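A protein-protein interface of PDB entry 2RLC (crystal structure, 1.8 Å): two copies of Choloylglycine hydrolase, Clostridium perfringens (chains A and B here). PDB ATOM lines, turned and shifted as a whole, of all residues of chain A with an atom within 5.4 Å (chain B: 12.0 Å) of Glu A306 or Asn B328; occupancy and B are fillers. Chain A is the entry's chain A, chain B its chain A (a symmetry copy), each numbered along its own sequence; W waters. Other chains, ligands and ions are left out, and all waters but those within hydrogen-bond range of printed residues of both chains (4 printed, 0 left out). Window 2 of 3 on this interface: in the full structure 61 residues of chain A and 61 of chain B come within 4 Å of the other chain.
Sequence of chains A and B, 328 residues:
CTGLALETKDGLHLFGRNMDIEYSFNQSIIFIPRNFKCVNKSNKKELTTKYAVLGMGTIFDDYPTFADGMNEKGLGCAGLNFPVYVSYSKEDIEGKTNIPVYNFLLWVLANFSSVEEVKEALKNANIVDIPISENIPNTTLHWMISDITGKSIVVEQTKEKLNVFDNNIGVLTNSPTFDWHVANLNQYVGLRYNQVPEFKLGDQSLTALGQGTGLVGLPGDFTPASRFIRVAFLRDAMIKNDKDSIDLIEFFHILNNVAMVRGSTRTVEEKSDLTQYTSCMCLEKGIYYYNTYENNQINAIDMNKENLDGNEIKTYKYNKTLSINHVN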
ATOM      1  N   PHE A  31       6.096 -33.302   9.297  1.00  0.00           N
ATOM      2  CA  PHE A  31       5.036 -32.325   9.496  1.00  0.00           C
ATOM      3  C   PHE A  31       3.795 -32.745   8.708  1.00  0.00           C
ATOM      4  O   PHE A  31       3.879 -33.036   7.512  1.00  0.00           O
ATOM      5  CB  PHE A  31       5.493 -30.921   9.074  1.00  0.00           C
ATOM      6  CG  PHE A  31       4.374 -29.915   9.000  1.00  0.00           C
ATOM      7  CD1 PHE A  31       3.862 -29.335  10.157  1.00  0.00           C
ATOM      8  CD2 PHE A  31       3.822 -29.561   7.770  1.00  0.00           C
ATOM      9  CE1 PHE A  31       2.820 -28.414  10.091  1.00  0.00           C
ATOM     10  CE2 PHE A  31       2.778 -28.640   7.693  1.00  0.00           C
ATOM     11  CZ  PHE A  31       2.276 -28.066   8.854  1.00  0.00           C
ATOM     12  N   ALA A 300      16.349 -27.187  15.158  1.00  0.00           N
ATOM     13  CA  ALA A 300      15.003 -26.697  15.437  1.00  0.00           C
ATOM     14  C   ALA A 300      14.133 -26.688  14.191  1.00  0.00           C
ATOM     15  O   ALA A 300      14.515 -26.130  13.159  1.00  0.00           O
ATOM     16  CB  ALA A 300      15.062 -25.306  16.047  1.00  0.00           C
ATOM     17  N   ILE A 301      12.966 -27.314  14.300  1.00  0.00           N
ATOM     18  CA  ILE A 301      11.939 -27.233  13.267  1.00  0.00           C
ATOM     19  C   ILE A 301      10.709 -26.579  13.888  1.00  0.00           C
ATOM     20  O   ILE A 301      10.146 -27.086  14.861  1.00  0.00           O
ATOM     21  CB  ILE A 301      11.584 -28.619  12.657  1.00  0.00           C
ATOM     22  CG1 ILE A 301      12.809 -29.269  12.002  1.00  0.00           C
ATOM     23  CG2 ILE A 301      10.470 -28.485  11.619  1.00  0.00           C
ATOM     24  CD1 ILE A 301      13.526 -30.282  12.879  1.00  0.00           C
ATOM     25  N   ASP A 302      10.321 -25.438  13.328  1.00  0.00           N
ATOM     26  CA  ASP A 302       9.203 -24.647  13.830  1.00  0.00           C
ATOM     27  C   ASP A 302       7.997 -24.862  12.924  1.00  0.00           C
ATOM     28  O   ASP A 302       7.992 -24.422  11.773  1.00  0.00           O
ATOM     29  CB  ASP A 302       9.601 -23.163  13.874  1.00  0.00           C
ATOM     30  CG  ASP A 302       8.559 -22.277  14.551  1.00  0.00           C
ATOM     31  OD1 ASP A 302       7.393 -22.695  14.714  1.00  0.00           O
ATOM     32  OD2 ASP A 302       8.917 -21.138  14.916  1.00  0.00           O
ATOM     33  N   MET A 303       6.974 -25.534  13.448  1.00  0.00           N
ATOM     34  CA  MET A 303       5.764 -25.819  12.671  1.00  0.00           C
ATOM     35  C   MET A 303       5.014 -24.558  12.240  1.00  0.00           C
ATOM     36  O   MET A 303       4.264 -24.587  11.265  1.00  0.00           O
ATOM     37  CB  MET A 303       4.830 -26.775  13.424  1.00  0.00           C
ATOM     38  CG  MET A 303       4.162 -26.200  14.664  1.00  0.00           C
ATOM     39  SD  MET A 303       3.211 -27.583  15.657  1.00  0.00           S
ATOM     40  CE  MET A 303       2.043 -28.190  14.236  1.00  0.00           C
ATOM     41  N   ASN A 304       5.223 -23.462  12.964  1.00  0.00           N
ATOM     42  CA  ASN A 304       4.556 -22.196  12.660  1.00  0.00           C
ATOM     43  C   ASN A 304       5.166 -21.455  11.472  1.00  0.00           C
ATOM     44  O   ASN A 304       4.621 -20.452  11.014  1.00  0.00           O
ATOM     45  CB  ASN A 304       4.500 -21.299  13.899  1.00  0.00           C
ATOM     46  CG  ASN A 304       3.622 -21.873  14.992  1.00  0.00           C
ATOM     47  OD1 ASN A 304       4.098 -22.191  16.081  1.00  0.00           O
ATOM     48  ND2 ASN A 304       2.334 -22.022  14.703  1.00  0.00           N
ATOM     49  N   LYS A 305       6.297 -21.955  10.977  1.00  0.00           N
ATOM     50  CA  LYS A 305       6.888 -21.446   9.742  1.00  0.00           C
ATOM     51  C   LYS A 305       6.257 -22.130   8.528  1.00  0.00           C
ATOM     52  O   LYS A 305       6.432 -21.686   7.391  1.00  0.00           O
ATOM     53  CB  LYS A 305       8.406 -21.636   9.750  1.00  0.00           C
ATOM     54  CG  LYS A 305       9.131 -20.720  10.718  1.00  0.00           C
ATOM     55  CD  LYS A 305      10.600 -21.083  10.824  1.00  0.00           C
ATOM     56  CE  LYS A 305      11.355 -20.128  11.734  1.00  0.00           C
ATOM     57  NZ  LYS A 305      11.558 -18.789  11.110  1.00  0.00           N
ATOM     58  N   GLU A 306       5.518 -23.207   8.785  1.00  0.00           N
ATOM     59  CA  GLU A 306       4.813 -23.949   7.745  1.00  0.00           C
ATOM     60  C   GLU A 306       3.432 -23.354   7.499  1.00  0.00           C
ATOM     61  O   GLU A 306       2.907 -22.612   8.329  1.00  0.00           O
ATOM     62  CB  GLU A 306       4.636 -25.415   8.152  1.00  0.00           C
ATOM     63  CG  GLU A 306       5.871 -26.088   8.727  1.00  0.00           C
ATOM     64  CD  GLU A 306       6.748 -26.717   7.672  1.00  0.00           C
ATOM     65  OE1 GLU A 306       6.779 -26.220   6.523  1.00  0.00           O
ATOM     66  OE2 GLU A 306       7.422 -27.716   8.001  1.00  0.00           O
ATOM     67  N   ASN A 307       2.852 -23.688   6.351  1.00  0.00           N
ATOM     68  CA  ASN A 307       1.443 -23.425   6.107  1.00  0.00           C
ATOM     69  C   ASN A 307       0.627 -24.528   6.771  1.00  0.00           C
ATOM     70  O   ASN A 307       0.614 -25.668   6.307  1.00  0.00           O
ATOM     71  CB  ASN A 307       1.148 -23.349   4.606  1.00  0.00           C
ATOM     72  CG  ASN A 307      -0.317 -23.059   4.305  1.00  0.00           C
ATOM     73  OD1 ASN A 307      -1.059 -22.569   5.160  1.00  0.00           O
ATOM     74  ND2 ASN A 307      -0.736 -23.357   3.078  1.00  0.00           N
ATOM     75  N   LEU A 308      -0.040 -24.178   7.869  1.00  0.00           N
ATOM     76  CA  LEU A 308      -0.817 -25.140   8.651  1.00  0.00           C
ATOM     77  C   LEU A 308      -2.049 -25.630   7.890  1.00  0.00           C
ATOM     78  O   LEU A 308      -2.580 -26.707   8.174  1.00  0.00           O
ATOM     79  CB  LEU A 308      -1.204 -24.549  10.013  1.00  0.00           C
ATOM     80  CG  LEU A 308      -0.067 -24.085  10.940  1.00  0.00           C
ATOM     81  CD1 LEU A 308      -0.623 -23.512  12.233  1.00  0.00           C
ATOM     82  CD2 LEU A 308       0.928 -25.207  11.239  1.00  0.00           C
ATOM     83  N   LYS A 314       5.169 -32.727   4.894  1.00  0.00           N
ATOM     84  CA  LYS A 314       6.541 -32.275   4.714  1.00  0.00           C
ATOM     85  C   LYS A 314       7.459 -33.037   5.658  1.00  0.00           C
ATOM     86  O   LYS A 314       7.112 -33.265   6.819  1.00  0.00           O
ATOM     87  CB  LYS A 314       6.649 -30.768   4.952  1.00  0.00           C
ATOM     88  CG  LYS A 314       5.816 -29.930   3.976  1.00  0.00           C
ATOM     89  CD  LYS A 314       5.984 -28.439   4.207  1.00  0.00           C
ATOM     90  CE  LYS A 314       7.279 -27.916   3.597  1.00  0.00           C
ATOM     91  NZ  LYS A 314       7.386 -26.442   3.734  1.00  0.00           N
ATOM     92  N   TYR A 316      11.723 -33.638   7.027  1.00  0.00           N
ATOM     93  CA  TYR A 316      13.043 -33.042   7.180  1.00  0.00           C
ATOM     94  C   TYR A 316      14.038 -34.123   7.558  1.00  0.00           C
ATOM     95  O   TYR A 316      13.750 -34.973   8.400  1.00  0.00           O
ATOM     96  CB  TYR A 316      13.014 -31.929   8.230  1.00  0.00           C
ATOM     97  CG  TYR A 316      12.066 -30.817   7.861  1.00  0.00           C
ATOM     98  CD1 TYR A 316      12.490 -29.759   7.062  1.00  0.00           C
ATOM     99  CD2 TYR A 316      10.734 -30.836   8.284  1.00  0.00           C
ATOM    100  CE1 TYR A 316      11.626 -28.741   6.702  1.00  0.00           C
ATOM    101  CE2 TYR A 316       9.857 -29.816   7.926  1.00  0.00           C
ATOM    102  CZ  TYR A 316      10.314 -28.774   7.136  1.00  0.00           C
ATOM    103  OH  TYR A 316       9.470 -27.756   6.766  1.00  0.00           O
ATOM    104  N   ILE B 324      21.990 -22.924  17.962  1.00  0.00           N
ATOM    105  CA  ILE B 324      20.957 -23.802  17.412  1.00  0.00           C
ATOM    106  C   ILE B 324      20.930 -23.732  15.889  1.00  0.00           C
ATOM    107  O   ILE B 324      21.047 -22.653  15.309  1.00  0.00           O
ATOM    108  CB  ILE B 324      19.557 -23.428  17.973  1.00  0.00           C
ATOM    109  CG1 ILE B 324      19.521 -23.613  19.494  1.00  0.00           C
ATOM    110  CG2 ILE B 324      18.450 -24.253  17.304  1.00  0.00           C
ATOM    111  CD1 ILE B 324      18.448 -22.797  20.186  1.00  0.00           C
ATOM    112  N   ASN B 325      20.782 -24.890  15.252  1.00  0.00           N
ATOM    113  CA  ASN B 325      20.578 -24.957  13.814  1.00  0.00           C
ATOM    114  C   ASN B 325      19.085 -24.869  13.491  1.00  0.00           C
ATOM    115  O   ASN B 325      18.337 -25.814  13.728  1.00  0.00           O
ATOM    116  CB  ASN B 325      21.192 -26.242  13.244  1.00  0.00           C
ATOM    117  CG  ASN B 325      20.906 -26.424  11.762  1.00  0.00           C
ATOM    118  OD1 ASN B 325      21.087 -25.507  10.965  1.00  0.00           O
ATOM    119  ND2 ASN B 325      20.455 -27.618  11.389  1.00  0.00           N
ATOM    120  N   HIS B 326      18.657 -23.725  12.966  1.00  0.00           N
ATOM    121  CA  HIS B 326      17.262 -23.537  12.572  1.00  0.00           C
ATOM    122  C   HIS B 326      17.018 -24.135  11.189  1.00  0.00           C
ATOM    123  O   HIS B 326      17.362 -23.538  10.165  1.00  0.00           O
ATOM    124  CB  HIS B 326      16.873 -22.060  12.638  1.00  0.00           C
ATOM    125  CG  HIS B 326      16.928 -21.496  14.023  1.00  0.00           C
ATOM    126  ND1 HIS B 326      18.084 -20.980  14.569  1.00  0.00           N
ATOM    127  CD2 HIS B 326      15.980 -21.391  14.983  1.00  0.00           C
ATOM    128  CE1 HIS B 326      17.841 -20.570  15.801  1.00  0.00           C
ATOM    129  NE2 HIS B 326      16.574 -20.808  16.078  1.00  0.00           N
ATOM    130  N   VAL B 327      16.425 -25.326  11.187  1.00  0.00           N
ATOM    131  CA  VAL B 327      16.277 -26.153   9.983  1.00  0.00           C
ATOM    132  C   VAL B 327      15.372 -25.503   8.937  1.00  0.00           C
ATOM    133  O   VAL B 327      15.707 -25.471   7.749  1.00  0.00           O
ATOM    134  CB  VAL B 327      15.773 -27.579  10.341  1.00  0.00           C
ATOM    135  CG1 VAL B 327      15.554 -28.427   9.089  1.00  0.00           C
ATOM    136  CG2 VAL B 327      16.757 -28.271  11.278  1.00  0.00           C
ATOM    137  N   ASN B 328      14.232 -24.984   9.386  1.00  0.00           N
ATOM    138  CA  ASN B 328      13.291 -24.311   8.498  1.00  0.00           C
ATOM    139  C   ASN B 328      13.063 -22.856   8.894  1.00  0.00           C
ATOM    140  O   ASN B 328      12.336 -22.120   8.221  1.00  0.00           O
ATOM    141  CB  ASN B 328      11.967 -25.085   8.416  1.00  0.00           C
ATOM    142  CG  ASN B 328      11.140 -24.997   9.698  1.00  0.00           C
ATOM    143  OD1 ASN B 328      11.676 -24.847  10.798  1.00  0.00           O
ATOM    144  ND2 ASN B 328       9.822 -25.092   9.550  1.00  0.00           N
ATOM    145  OXT ASN B 328      13.600 -22.376   9.899  1.00  0.00           O
HETATM  146  O   HOH W   1      12.174 -19.509   7.766  1.00  0.00           O
HETATM  147  O   HOH W   2      14.665 -19.968  10.467  1.00  0.00           O
HETATM  148  O   HOH W   3       8.984 -24.655   6.837  1.00  0.00           O
HETATM  149  O   HOH W   4      13.816 -23.457  12.671  1.00  0.00           O
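The backbone NH of Asp A302 sits at hydrogen-bond distance from the side-chain amide oxygen of Asn B328 (2.9 Å).
The backbone NH (N) of Val B327 sits at hydrogen-bond distance from the backbone carbonyl oxygen (O) of Ala A300.
N of Ala A300 is in hydrogen-bond range of O of Asn B325 (2.8 Å).
The side-chain hydroxyl (OH) of Tyr A316 lies close to the side-chain carboxylate (OE1) of Glu A306.
The side-chain carboxylate of Asp A302 sits at hydrogen-bond distance from the backbone NH of Asn A304, at 2.9 Å.
The side-chain amino group of Lys A314 is in salt-bridge range of the side-chain carboxylate of Glu A306 (2.9 Å).
O of Ile B324 is in hydrogen-bond range of ND1 of His B326 (3.5 Å).
Ile B324 touches Ala A300.
His B326 touches Ala A300 (C to O, 3.8 Å).
OD1 of Asn B328 touches O of Ala A300, at 3.9 Å.
Ile A301 touches Val B327 (CG1 to CB, 3.8 Å).
Ile A301 touches Asn B328.
Lys A305 touches Asn B328 (CD to O, 3.3 Å).
Asn B328 touches Glu A306 (ND2 to OE2, 3.9 Å).
Tyr A316 touches Val B327 (CD1 to CG1, 3.9 Å).
Tyr A316 touches Asn B328.
Glu A306 touches just one residue of chain B: Asn B328 (3.9 Å).
Asn B328 touches just these residues of chain A: Ala A300, Ile A301, Asp A302, Lys A305, Glu A306 and Tyr A316.
No residue of chain B comes within 4 Å of Phe A31.
Ile A301 touches just these residues of chain B: Val B327 (3.8 Å) and Asn B328 (3.4 Å).
Of chain B, only Asn B328 (3.3 Å) comes within 4 Å of Lys A305.
No residue of chain B comes within 4 Å of Leu A308.
No residue of chain B comes within 4 Å of Lys A314.
Of the printed residues of chain A, His B326 touches Ala A300.
Of the printed residues of chain B, Tyr A316 touches Val B327 (3.9 Å) and Asn B328 (3.9 Å).
Of the printed residues of chain A, Ile B324 touches Ala A300 (3.8 Å).
Printed residues of chain A within 4 Å of Val B327: Ala A300, Ile A301 and Tyr A316.
The nearest residue of chain A that does not touch Asn B328 is Met A303 (4.8 Å).
The nearest printed residue of chain A that does not touch Val B327 is Asp A302 (6.5 Å).
Of the 12 printed residues of chain A, 6 touch a printed residue of chain B.
Printed residues of chain A that touch a printed residue of chain B: Ala A300, Ile A301, Asp A302, Lys A305, Glu A306 and Tyr A316.
Hydrophobic or aromatic side chains of chain B within 4 Å of the printed part of chain A: Ile B324 and Val B327.
No position is printed for both chains.
Of the 12 pairs that touch across the chains among the printed residues, none has its exchanged pair printed and touching as well.
Water W1 lies within hydrogen-bond range of the chain-end carboxylate of Asn B328 (2.7 Å) and the side-chain amino group of Lys A305 (3.5 Å).
Water W2 lies within hydrogen-bond range of OXT of Asn B328 (2.7 Å) and NZ of Lys A305 (3.4 Å).
Water W3 lies within hydrogen-bond range of the side-chain carboxylate (OE1) of Glu A306 (2.7 Å), the side-chain amide nitrogen (ND2) of Asn B328 (2.9 Å) and the side-chain hydroxyl (OH) of Tyr A316 (3.1 Å).
Water W4 lies within hydrogen-bond range of O of Ala A300 (2.8 Å) and OXT of Asn B328 (3.0 Å).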
